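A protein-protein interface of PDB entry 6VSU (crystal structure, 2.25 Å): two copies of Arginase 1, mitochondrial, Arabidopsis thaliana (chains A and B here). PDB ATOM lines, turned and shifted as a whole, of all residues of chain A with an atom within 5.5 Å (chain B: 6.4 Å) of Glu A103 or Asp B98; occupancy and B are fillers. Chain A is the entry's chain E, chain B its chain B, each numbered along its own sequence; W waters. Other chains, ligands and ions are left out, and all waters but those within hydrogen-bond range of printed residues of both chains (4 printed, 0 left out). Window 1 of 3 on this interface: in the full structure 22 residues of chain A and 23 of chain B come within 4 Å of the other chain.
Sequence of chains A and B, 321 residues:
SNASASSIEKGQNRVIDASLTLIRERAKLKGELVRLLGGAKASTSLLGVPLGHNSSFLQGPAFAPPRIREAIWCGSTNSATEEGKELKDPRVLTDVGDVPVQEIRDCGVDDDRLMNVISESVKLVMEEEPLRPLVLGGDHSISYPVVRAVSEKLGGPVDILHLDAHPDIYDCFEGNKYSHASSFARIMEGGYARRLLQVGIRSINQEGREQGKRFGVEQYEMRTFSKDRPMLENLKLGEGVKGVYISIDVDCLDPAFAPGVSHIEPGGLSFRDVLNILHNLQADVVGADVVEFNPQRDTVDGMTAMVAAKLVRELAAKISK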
ATOM      1  N   VAL A  15      22.678   5.694   4.251  1.00  0.00           N
ATOM      2  CA  VAL A  15      22.956   6.664   3.153  1.00  0.00           C
ATOM      3  C   VAL A  15      22.274   6.185   1.846  1.00  0.00           C
ATOM      4  O   VAL A  15      21.663   7.025   1.119  1.00  0.00           O
ATOM      5  CB  VAL A  15      24.466   6.865   3.015  1.00  0.00           C
ATOM      6  CG1 VAL A  15      24.813   7.696   1.805  1.00  0.00           C
ATOM      7  CG2 VAL A  15      25.049   7.484   4.265  1.00  0.00           C
ATOM      8  N   PRO A 100      23.099  10.464  -6.078  1.00  0.00           N
ATOM      9  CA  PRO A 100      24.259  10.980  -5.350  1.00  0.00           C
ATOM     10  C   PRO A 100      25.403   9.957  -5.224  1.00  0.00           C
ATOM     11  O   PRO A 100      25.708   9.488  -4.168  1.00  0.00           O
ATOM     12  CB  PRO A 100      23.649  11.378  -4.004  1.00  0.00           C
ATOM     13  CG  PRO A 100      22.445  10.453  -3.838  1.00  0.00           C
ATOM     14  CD  PRO A 100      21.939  10.167  -5.232  1.00  0.00           C
ATOM     15  N   VAL A 101      26.024   9.676  -6.351  1.00  0.00           N
ATOM     16  CA  VAL A 101      27.061   8.612  -6.530  1.00  0.00           C
ATOM     17  C   VAL A 101      28.254   8.897  -5.642  1.00  0.00           C
ATOM     18  O   VAL A 101      28.751   7.948  -4.991  1.00  0.00           O
ATOM     19  CB  VAL A 101      27.532   8.514  -7.997  1.00  0.00           C
ATOM     20  CG1 VAL A 101      28.742   7.615  -8.142  1.00  0.00           C
ATOM     21  CG2 VAL A 101      26.395   8.044  -8.878  1.00  0.00           C
ATOM     22  N   GLN A 102      28.766  10.126  -5.696  1.00  0.00           N
ATOM     23  CA  GLN A 102      30.075  10.401  -5.065  1.00  0.00           C
ATOM     24  C   GLN A 102      29.944  10.182  -3.569  1.00  0.00           C
ATOM     25  O   GLN A 102      30.919   9.747  -2.969  1.00  0.00           O
ATOM     26  CB  GLN A 102      30.653  11.758  -5.470  1.00  0.00           C
ATOM     27  CG  GLN A 102      30.965  11.861  -6.955  1.00  0.00           C
ATOM     28  CD  GLN A 102      31.779  10.670  -7.410  1.00  0.00           C
ATOM     29  OE1 GLN A 102      32.765  10.313  -6.769  1.00  0.00           O
ATOM     30  NE2 GLN A 102      31.388  10.084  -8.530  1.00  0.00           N
ATOM     31  N   GLU A 103      28.822  10.627  -3.000  1.00  0.00           N
ATOM     32  CA  GLU A 103      28.524  10.526  -1.547  1.00  0.00           C
ATOM     33  C   GLU A 103      28.398   9.053  -1.143  1.00  0.00           C
ATOM     34  O   GLU A 103      28.911   8.700  -0.078  1.00  0.00           O
ATOM     35  CB  GLU A 103      27.286  11.362  -1.220  1.00  0.00           C
ATOM     36  CG  GLU A 103      27.503  12.859  -1.360  1.00  0.00           C
ATOM     37  CD  GLU A 103      27.304  13.478  -2.737  1.00  0.00           C
ATOM     38  OE1 GLU A 103      27.003  12.744  -3.693  1.00  0.00           O
ATOM     39  OE2 GLU A 103      27.454  14.698  -2.845  1.00  0.00           O
ATOM     40  N   ILE A 104      27.741   8.236  -1.970  1.00  0.00           N
ATOM     41  CA  ILE A 104      27.635   6.774  -1.701  1.00  0.00           C
ATOM     42  C   ILE A 104      29.035   6.136  -1.744  1.00  0.00           C
ATOM     43  O   ILE A 104      29.421   5.429  -0.776  1.00  0.00           O
ATOM     44  CB  ILE A 104      26.668   6.129  -2.674  1.00  0.00           C
ATOM     45  CG1 ILE A 104      25.245   6.663  -2.456  1.00  0.00           C
ATOM     46  CG2 ILE A 104      26.761   4.612  -2.532  1.00  0.00           C
ATOM     47  CD1 ILE A 104      24.296   6.201  -3.527  1.00  0.00           C
ATOM     48  N   ARG A 105      29.842   6.483  -2.745  1.00  0.00           N
ATOM     49  CA  ARG A 105      31.228   5.949  -2.829  1.00  0.00           C
ATOM     50  C   ARG A 105      31.999   6.410  -1.599  1.00  0.00           C
ATOM     51  O   ARG A 105      32.763   5.618  -1.038  1.00  0.00           O
ATOM     52  CB  ARG A 105      31.975   6.489  -4.044  1.00  0.00           C
ATOM     53  CG  ARG A 105      31.420   6.106  -5.399  1.00  0.00           C
ATOM     54  CD  ARG A 105      32.348   6.633  -6.494  1.00  0.00           C
ATOM     55  NE  ARG A 105      33.755   6.129  -6.425  1.00  0.00           N
ATOM     56  CZ  ARG A 105      34.838   6.824  -6.786  1.00  0.00           C
ATOM     57  NH1 ARG A 105      34.712   8.087  -7.188  1.00  0.00           N
ATOM     58  NH2 ARG A 105      36.033   6.248  -6.762  1.00  0.00           N
ATOM     59  N   ASP A 106      31.802   7.671  -1.221  1.00  0.00           N
ATOM     60  CA  ASP A 106      32.582   8.341  -0.140  1.00  0.00           C
ATOM     61  C   ASP A 106      32.319   7.673   1.212  1.00  0.00           C
ATOM     62  O   ASP A 106      33.201   7.813   2.095  1.00  0.00           O
ATOM     63  CB  ASP A 106      32.358   9.860  -0.070  1.00  0.00           C
ATOM     64  CG  ASP A 106      33.477  10.567   0.688  1.00  0.00           C
ATOM     65  OD1 ASP A 106      34.595  10.634   0.126  1.00  0.00           O
ATOM     66  OD2 ASP A 106      33.256  11.016   1.851  1.00  0.00           O
ATOM     67  N   CYS A 107      31.200   6.965   1.410  1.00  0.00           N
ATOM     68  CA  CYS A 107      31.011   6.230   2.686  1.00  0.00           C
ATOM     69  C   CYS A 107      31.419   4.750   2.562  1.00  0.00           C
ATOM     70  O   CYS A 107      31.142   3.995   3.488  1.00  0.00           O
ATOM     71  CB  CYS A 107      29.605   6.422   3.237  1.00  0.00           C
ATOM     72  SG  CYS A 107      28.325   5.581   2.287  1.00  0.00           S
ATOM     73  N   LEU B  22      19.276  13.112   3.971  1.00  0.00           N
ATOM     74  CA  LEU B  22      20.518  12.556   3.361  1.00  0.00           C
ATOM     75  C   LEU B  22      21.769  13.247   3.963  1.00  0.00           C
ATOM     76  O   LEU B  22      22.765  12.571   4.199  1.00  0.00           O
ATOM     77  CB  LEU B  22      20.372  12.693   1.841  1.00  0.00           C
ATOM     78  CG  LEU B  22      21.565  12.294   0.990  1.00  0.00           C
ATOM     79  CD1 LEU B  22      22.024  10.878   1.287  1.00  0.00           C
ATOM     80  CD2 LEU B  22      21.185  12.443  -0.458  1.00  0.00           C
ATOM     81  N   ILE B  23      21.738  14.552   4.213  1.00  0.00           N
ATOM     82  CA  ILE B  23      22.898  15.259   4.841  1.00  0.00           C
ATOM     83  C   ILE B  23      23.075  14.719   6.255  1.00  0.00           C
ATOM     84  O   ILE B  23      24.252  14.530   6.651  1.00  0.00           O
ATOM     85  CB  ILE B  23      22.741  16.787   4.850  1.00  0.00           C
ATOM     86  CG1 ILE B  23      22.525  17.328   3.435  1.00  0.00           C
ATOM     87  CG2 ILE B  23      23.933  17.447   5.558  1.00  0.00           C
ATOM     88  CD1 ILE B  23      23.662  16.964   2.500  1.00  0.00           C
ATOM     89  N   ARG B  26      24.833  11.193   6.226  1.00  0.00           N
ATOM     90  CA  ARG B  26      26.240  11.373   5.786  1.00  0.00           C
ATOM     91  C   ARG B  26      27.061  12.002   6.925  1.00  0.00           C
ATOM     92  O   ARG B  26      28.176  11.519   7.165  1.00  0.00           O
ATOM     93  CB  ARG B  26      26.287  12.174   4.475  1.00  0.00           C
ATOM     94  CG  ARG B  26      26.127  11.287   3.252  1.00  0.00           C
ATOM     95  CD  ARG B  26      25.526  11.899   2.009  1.00  0.00           C
ATOM     96  NE  ARG B  26      25.771  13.313   1.647  1.00  0.00           N
ATOM     97  CZ  ARG B  26      25.270  13.934   0.563  1.00  0.00           C
ATOM     98  NH1 ARG B  26      24.560  13.267  -0.337  1.00  0.00           N
ATOM     99  NH2 ARG B  26      25.513  15.217   0.360  1.00  0.00           N
ATOM    100  N   LEU B  46      33.553  19.337   5.029  1.00  0.00           N
ATOM    101  CA  LEU B  46      33.158  20.059   3.797  1.00  0.00           C
ATOM    102  C   LEU B  46      31.669  19.845   3.592  1.00  0.00           C
ATOM    103  O   LEU B  46      31.210  18.690   3.766  1.00  0.00           O
ATOM    104  CB  LEU B  46      33.938  19.539   2.585  1.00  0.00           C
ATOM    105  CG  LEU B  46      35.461  19.611   2.686  1.00  0.00           C
ATOM    106  CD1 LEU B  46      36.120  19.190   1.388  1.00  0.00           C
ATOM    107  CD2 LEU B  46      35.911  21.023   3.055  1.00  0.00           C
ATOM    108  N   LEU B  47      30.970  20.916   3.232  1.00  0.00           N
ATOM    109  CA  LEU B  47      29.578  20.899   2.758  1.00  0.00           C
ATOM    110  C   LEU B  47      29.520  21.688   1.445  1.00  0.00           C
ATOM    111  O   LEU B  47      29.797  22.890   1.430  1.00  0.00           O
ATOM    112  CB  LEU B  47      28.666  21.475   3.844  1.00  0.00           C
ATOM    113  CG  LEU B  47      27.159  21.464   3.548  1.00  0.00           C
ATOM    114  CD1 LEU B  47      26.608  20.053   3.526  1.00  0.00           C
ATOM    115  CD2 LEU B  47      26.394  22.281   4.602  1.00  0.00           C
ATOM    116  N   GLY B  48      29.176  21.041   0.346  1.00  0.00           N
ATOM    117  CA  GLY B  48      29.020  21.790  -0.901  1.00  0.00           C
ATOM    118  C   GLY B  48      27.608  22.340  -1.015  1.00  0.00           C
ATOM    119  O   GLY B  48      26.648  21.659  -0.551  1.00  0.00           O
ATOM    120  N   VAL B  49      27.491  23.514  -1.649  1.00  0.00           N
ATOM    121  CA  VAL B  49      26.202  24.186  -1.929  1.00  0.00           C
ATOM    122  C   VAL B  49      26.330  24.645  -3.365  1.00  0.00           C
ATOM    123  O   VAL B  49      26.797  25.749  -3.660  1.00  0.00           O
ATOM    124  CB  VAL B  49      25.943  25.336  -0.933  1.00  0.00           C
ATOM    125  CG1 VAL B  49      24.607  26.023  -1.188  1.00  0.00           C
ATOM    126  CG2 VAL B  49      26.054  24.835   0.508  1.00  0.00           C
ATOM    127  N   PRO B  50      25.990  23.736  -4.292  1.00  0.00           N
ATOM    128  CA  PRO B  50      26.163  23.997  -5.721  1.00  0.00           C
ATOM    129  C   PRO B  50      25.055  24.927  -6.238  1.00  0.00           C
ATOM    130  O   PRO B  50      24.075  24.426  -6.800  1.00  0.00           O
ATOM    131  CB  PRO B  50      26.110  22.587  -6.361  1.00  0.00           C
ATOM    132  CG  PRO B  50      25.359  21.732  -5.376  1.00  0.00           C
ATOM    133  CD  PRO B  50      25.602  22.351  -4.007  1.00  0.00           C
ATOM    134  N   PRO B  65      31.828  22.865  -6.525  1.00  0.00           N
ATOM    135  CA  PRO B  65      32.215  22.002  -5.425  1.00  0.00           C
ATOM    136  C   PRO B  65      32.745  20.651  -5.876  1.00  0.00           C
ATOM    137  O   PRO B  65      33.745  20.213  -5.346  1.00  0.00           O
ATOM    138  CB  PRO B  65      30.959  21.885  -4.568  1.00  0.00           C
ATOM    139  CG  PRO B  65      30.198  23.183  -4.891  1.00  0.00           C
ATOM    140  CD  PRO B  65      30.454  23.366  -6.379  1.00  0.00           C
ATOM    141  N   PRO B  66      32.194  19.968  -6.891  1.00  0.00           N
ATOM    142  CA  PRO B  66      32.832  18.741  -7.337  1.00  0.00           C
ATOM    143  C   PRO B  66      34.262  18.989  -7.849  1.00  0.00           C
ATOM    144  O   PRO B  66      35.117  18.182  -7.571  1.00  0.00           O
ATOM    145  CB  PRO B  66      31.840  18.223  -8.391  1.00  0.00           C
ATOM    146  CG  PRO B  66      30.504  18.843  -7.991  1.00  0.00           C
ATOM    147  CD  PRO B  66      30.888  20.218  -7.514  1.00  0.00           C
ATOM    148  N   ARG B  69      36.780  19.406  -4.919  1.00  0.00           N
ATOM    149  CA  ARG B  69      37.133  18.097  -4.297  1.00  0.00           C
ATOM    150  C   ARG B  69      38.154  17.384  -5.160  1.00  0.00           C
ATOM    151  O   ARG B  69      39.114  16.851  -4.625  1.00  0.00           O
ATOM    152  CB  ARG B  69      35.948  17.143  -4.173  1.00  0.00           C
ATOM    153  CG  ARG B  69      34.910  17.656  -3.206  1.00  0.00           C
ATOM    154  CD  ARG B  69      33.773  16.640  -3.068  1.00  0.00           C
ATOM    155  NE  ARG B  69      32.917  17.208  -2.023  1.00  0.00           N
ATOM    156  CZ  ARG B  69      31.851  17.975  -2.233  1.00  0.00           C
ATOM    157  NH1 ARG B  69      31.398  18.167  -3.463  1.00  0.00           N
ATOM    158  NH2 ARG B  69      31.169  18.444  -1.197  1.00  0.00           N
ATOM    159  N   ASP B  95      34.133  15.059   4.608  1.00  0.00           N
ATOM    160  CA  ASP B  95      33.276  15.645   3.569  1.00  0.00           C
ATOM    161  C   ASP B  95      31.885  15.027   3.687  1.00  0.00           C
ATOM    162  O   ASP B  95      31.768  13.786   3.512  1.00  0.00           O
ATOM    163  CB  ASP B  95      33.956  15.397   2.222  1.00  0.00           C
ATOM    164  CG  ASP B  95      33.251  16.045   1.044  1.00  0.00           C
ATOM    165  OD1 ASP B  95      32.285  16.769   1.262  1.00  0.00           O
ATOM    166  OD2 ASP B  95      33.700  15.816  -0.084  1.00  0.00           O
ATOM    167  N   VAL B  96      30.871  15.839   3.953  1.00  0.00           N
ATOM    168  CA  VAL B  96      29.476  15.344   4.011  1.00  0.00           C
ATOM    169  C   VAL B  96      28.817  15.550   2.645  1.00  0.00           C
ATOM    170  O   VAL B  96      27.667  15.165   2.504  1.00  0.00           O
ATOM    171  CB  VAL B  96      28.633  15.914   5.167  1.00  0.00           C
ATOM    172  CG1 VAL B  96      29.377  15.896   6.497  1.00  0.00           C
ATOM    173  CG2 VAL B  96      28.127  17.299   4.870  1.00  0.00           C
ATOM    174  N   GLY B  97      29.541  16.047   1.653  1.00  0.00           N
ATOM    175  CA  GLY B  97      29.055  16.116   0.271  1.00  0.00           C
ATOM    176  C   GLY B  97      28.199  17.352   0.035  1.00  0.00           C
ATOM    177  O   GLY B  97      28.443  18.363   0.659  1.00  0.00           O
ATOM    178  N   ASP B  98      27.335  17.283  -0.958  1.00  0.00           N
ATOM    179  CA  ASP B  98      26.654  18.431  -1.595  1.00  0.00           C
ATOM    180  C   ASP B  98      25.165  18.451  -1.196  1.00  0.00           C
ATOM    181  O   ASP B  98      24.534  17.437  -1.164  1.00  0.00           O
ATOM    182  CB  ASP B  98      26.828  18.363  -3.120  1.00  0.00           C
ATOM    183  CG  ASP B  98      28.155  18.889  -3.652  1.00  0.00           C
ATOM    184  OD1 ASP B  98      28.988  19.370  -2.824  1.00  0.00           O
ATOM    185  OD2 ASP B  98      28.345  18.857  -4.911  1.00  0.00           O
ATOM    186  N   VAL B  99      24.680  19.621  -0.818  1.00  0.00           N
ATOM    187  CA  VAL B  99      23.232  19.918  -0.710  1.00  0.00           C
ATOM    188  C   VAL B  99      22.689  19.770  -2.113  1.00  0.00           C
ATOM    189  O   VAL B  99      23.168  20.415  -3.025  1.00  0.00           O
ATOM    190  CB  VAL B  99      23.009  21.366  -0.186  1.00  0.00           C
ATOM    191  CG1 VAL B  99      21.536  21.755  -0.229  1.00  0.00           C
ATOM    192  CG2 VAL B  99      23.555  21.547   1.217  1.00  0.00           C
ATOM    193  N   PRO B 100      21.668  18.953  -2.346  1.00  0.00           N
ATOM    194  CA  PRO B 100      21.093  18.828  -3.690  1.00  0.00           C
ATOM    195  C   PRO B 100      20.184  20.020  -4.070  1.00  0.00           C
ATOM    196  O   PRO B 100      18.963  19.918  -4.250  1.00  0.00           O
ATOM    197  CB  PRO B 100      20.409  17.448  -3.588  1.00  0.00           C
ATOM    198  CG  PRO B 100      19.946  17.407  -2.132  1.00  0.00           C
ATOM    199  CD  PRO B 100      21.038  18.093  -1.345  1.00  0.00           C
ATOM    200  N   VAL B 101      20.848  21.152  -4.290  1.00  0.00           N
ATOM    201  CA  VAL B 101      20.230  22.480  -4.568  1.00  0.00           C
ATOM    202  C   VAL B 101      19.431  22.414  -5.860  1.00  0.00           C
ATOM    203  O   VAL B 101      18.325  22.871  -5.888  1.00  0.00           O
ATOM    204  CB  VAL B 101      21.357  23.515  -4.664  1.00  0.00           C
ATOM    205  CG1 VAL B 101      20.911  24.810  -5.343  1.00  0.00           C
ATOM    206  CG2 VAL B 101      21.960  23.729  -3.291  1.00  0.00           C
ATOM    207  N   LEU B 136      31.724  24.808   0.505  1.00  0.00           N
ATOM    208  CA  LEU B 136      32.195  25.013  -0.879  1.00  0.00           C
ATOM    209  C   LEU B 136      31.052  25.606  -1.683  1.00  0.00           C
ATOM    210  O   LEU B 136      29.965  24.907  -1.893  1.00  0.00           O
ATOM    211  CB  LEU B 136      32.596  23.683  -1.506  1.00  0.00           C
ATOM    212  CG  LEU B 136      33.599  22.804  -0.759  1.00  0.00           C
ATOM    213  CD1 LEU B 136      34.022  21.623  -1.625  1.00  0.00           C
ATOM    214  CD2 LEU B 136      34.820  23.595  -0.337  1.00  0.00           C
HETATM  215  O   HOH W   1      30.308  12.522   1.226  1.00  0.00           O
HETATM  216  O   HOH W   2      30.081  15.107  -3.109  1.00  0.00           O
HETATM  217  O   HOH W   3      35.244  12.283   3.723  1.00  0.00           O
HETATM  218  O   HOH W   4      24.557  10.250  -1.200  1.00  0.00           O
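Water W2 bridges OE2 of Glu A103 (2.7 Å) and NH1 of Arg B69 (3.4 Å). Water W1 lies within hydrogen-bond range of O of Asp B95 and OD2 of Asp A106. Water W3 lies within hydrogen-bond range of the side-chain carboxylate (OD2) of Asp A106 (3.0 Å) and the backbone NH (N) of Asp B95 (3.1 Å). Water W4 bridges NH1 of Arg B26 (3.1 Å) and O of Pro A100 (3.3 Å).
Of the 19 printed residues of chain B, 5 touch a printed residue of chain A. Hydrophobic or aromatic side chains of chain B within 4 Å of the printed part of chain A: Leu B22. Along chain B the printed residues that touch a printed residue of chain A span positions 22 to 98. Of the 9 printed residues of chain A, 3 touch a printed residue of chain B.
Glu A103 touches just these residues of chain B: Arg B26, Gly B97 and Asp B98. Printed residues of chain A within 4 Å of Leu B22: Val A15 (3.9 Å). Of the printed residues of chain A, Gly B97 touches Glu A103 (3.8 Å). Of the printed residues of chain B, Val A15 touches Leu B22. Printed residues of chain B within 4 Å of Asp A106: Asp B95 (3.6 Å). The nearest residue of chain B that does not touch Glu A103 is Val B96 (4.5 Å).
Positions printed for both chains: 100 and 101. Of the 5 pairs that touch across the chains among the printed residues, none has its exchanged pair printed and touching as well.
The guanidinium group (NH2) of Arg B69 lies within hydrogen-bond range of the backbone carbonyl oxygen (O) of Gly B97 (3.3 Å). OD2 of Asp B95 is in salt-bridge range of NE of Arg B69, at 2.5 Å. OD1 of Asp B98 lies within salt-bridge range of NH1 of Arg B69. O of Gly B97 is in hydrogen-bond range of N of Gly B48 (2.8 Å). The guanidinium group (NE) of Arg B26 sits at hydrogen-bond distance from the backbone carbonyl oxygen (O) of Val B96, at 2.8 Å. OD1 of Asp B95 is in hydrogen-bond range of N of Gly B97 (2.9 Å).
Among the printed residues, merely in contact across the chains: Val A15 with Leu B22 (3.9 Å), Glu A103 with Gly B97 (3.8 Å) and Asp A106 with Asp B95 (3.6 Å).
The backbone NH of Asp B98 is in hydrogen-bond range of the side-chain carboxylate of Glu A103, 3.2 Å away. The guanidinium group (NH2) of Arg B26 is in salt-bridge range of the side-chain carboxylate (OE2) of Glu A103.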
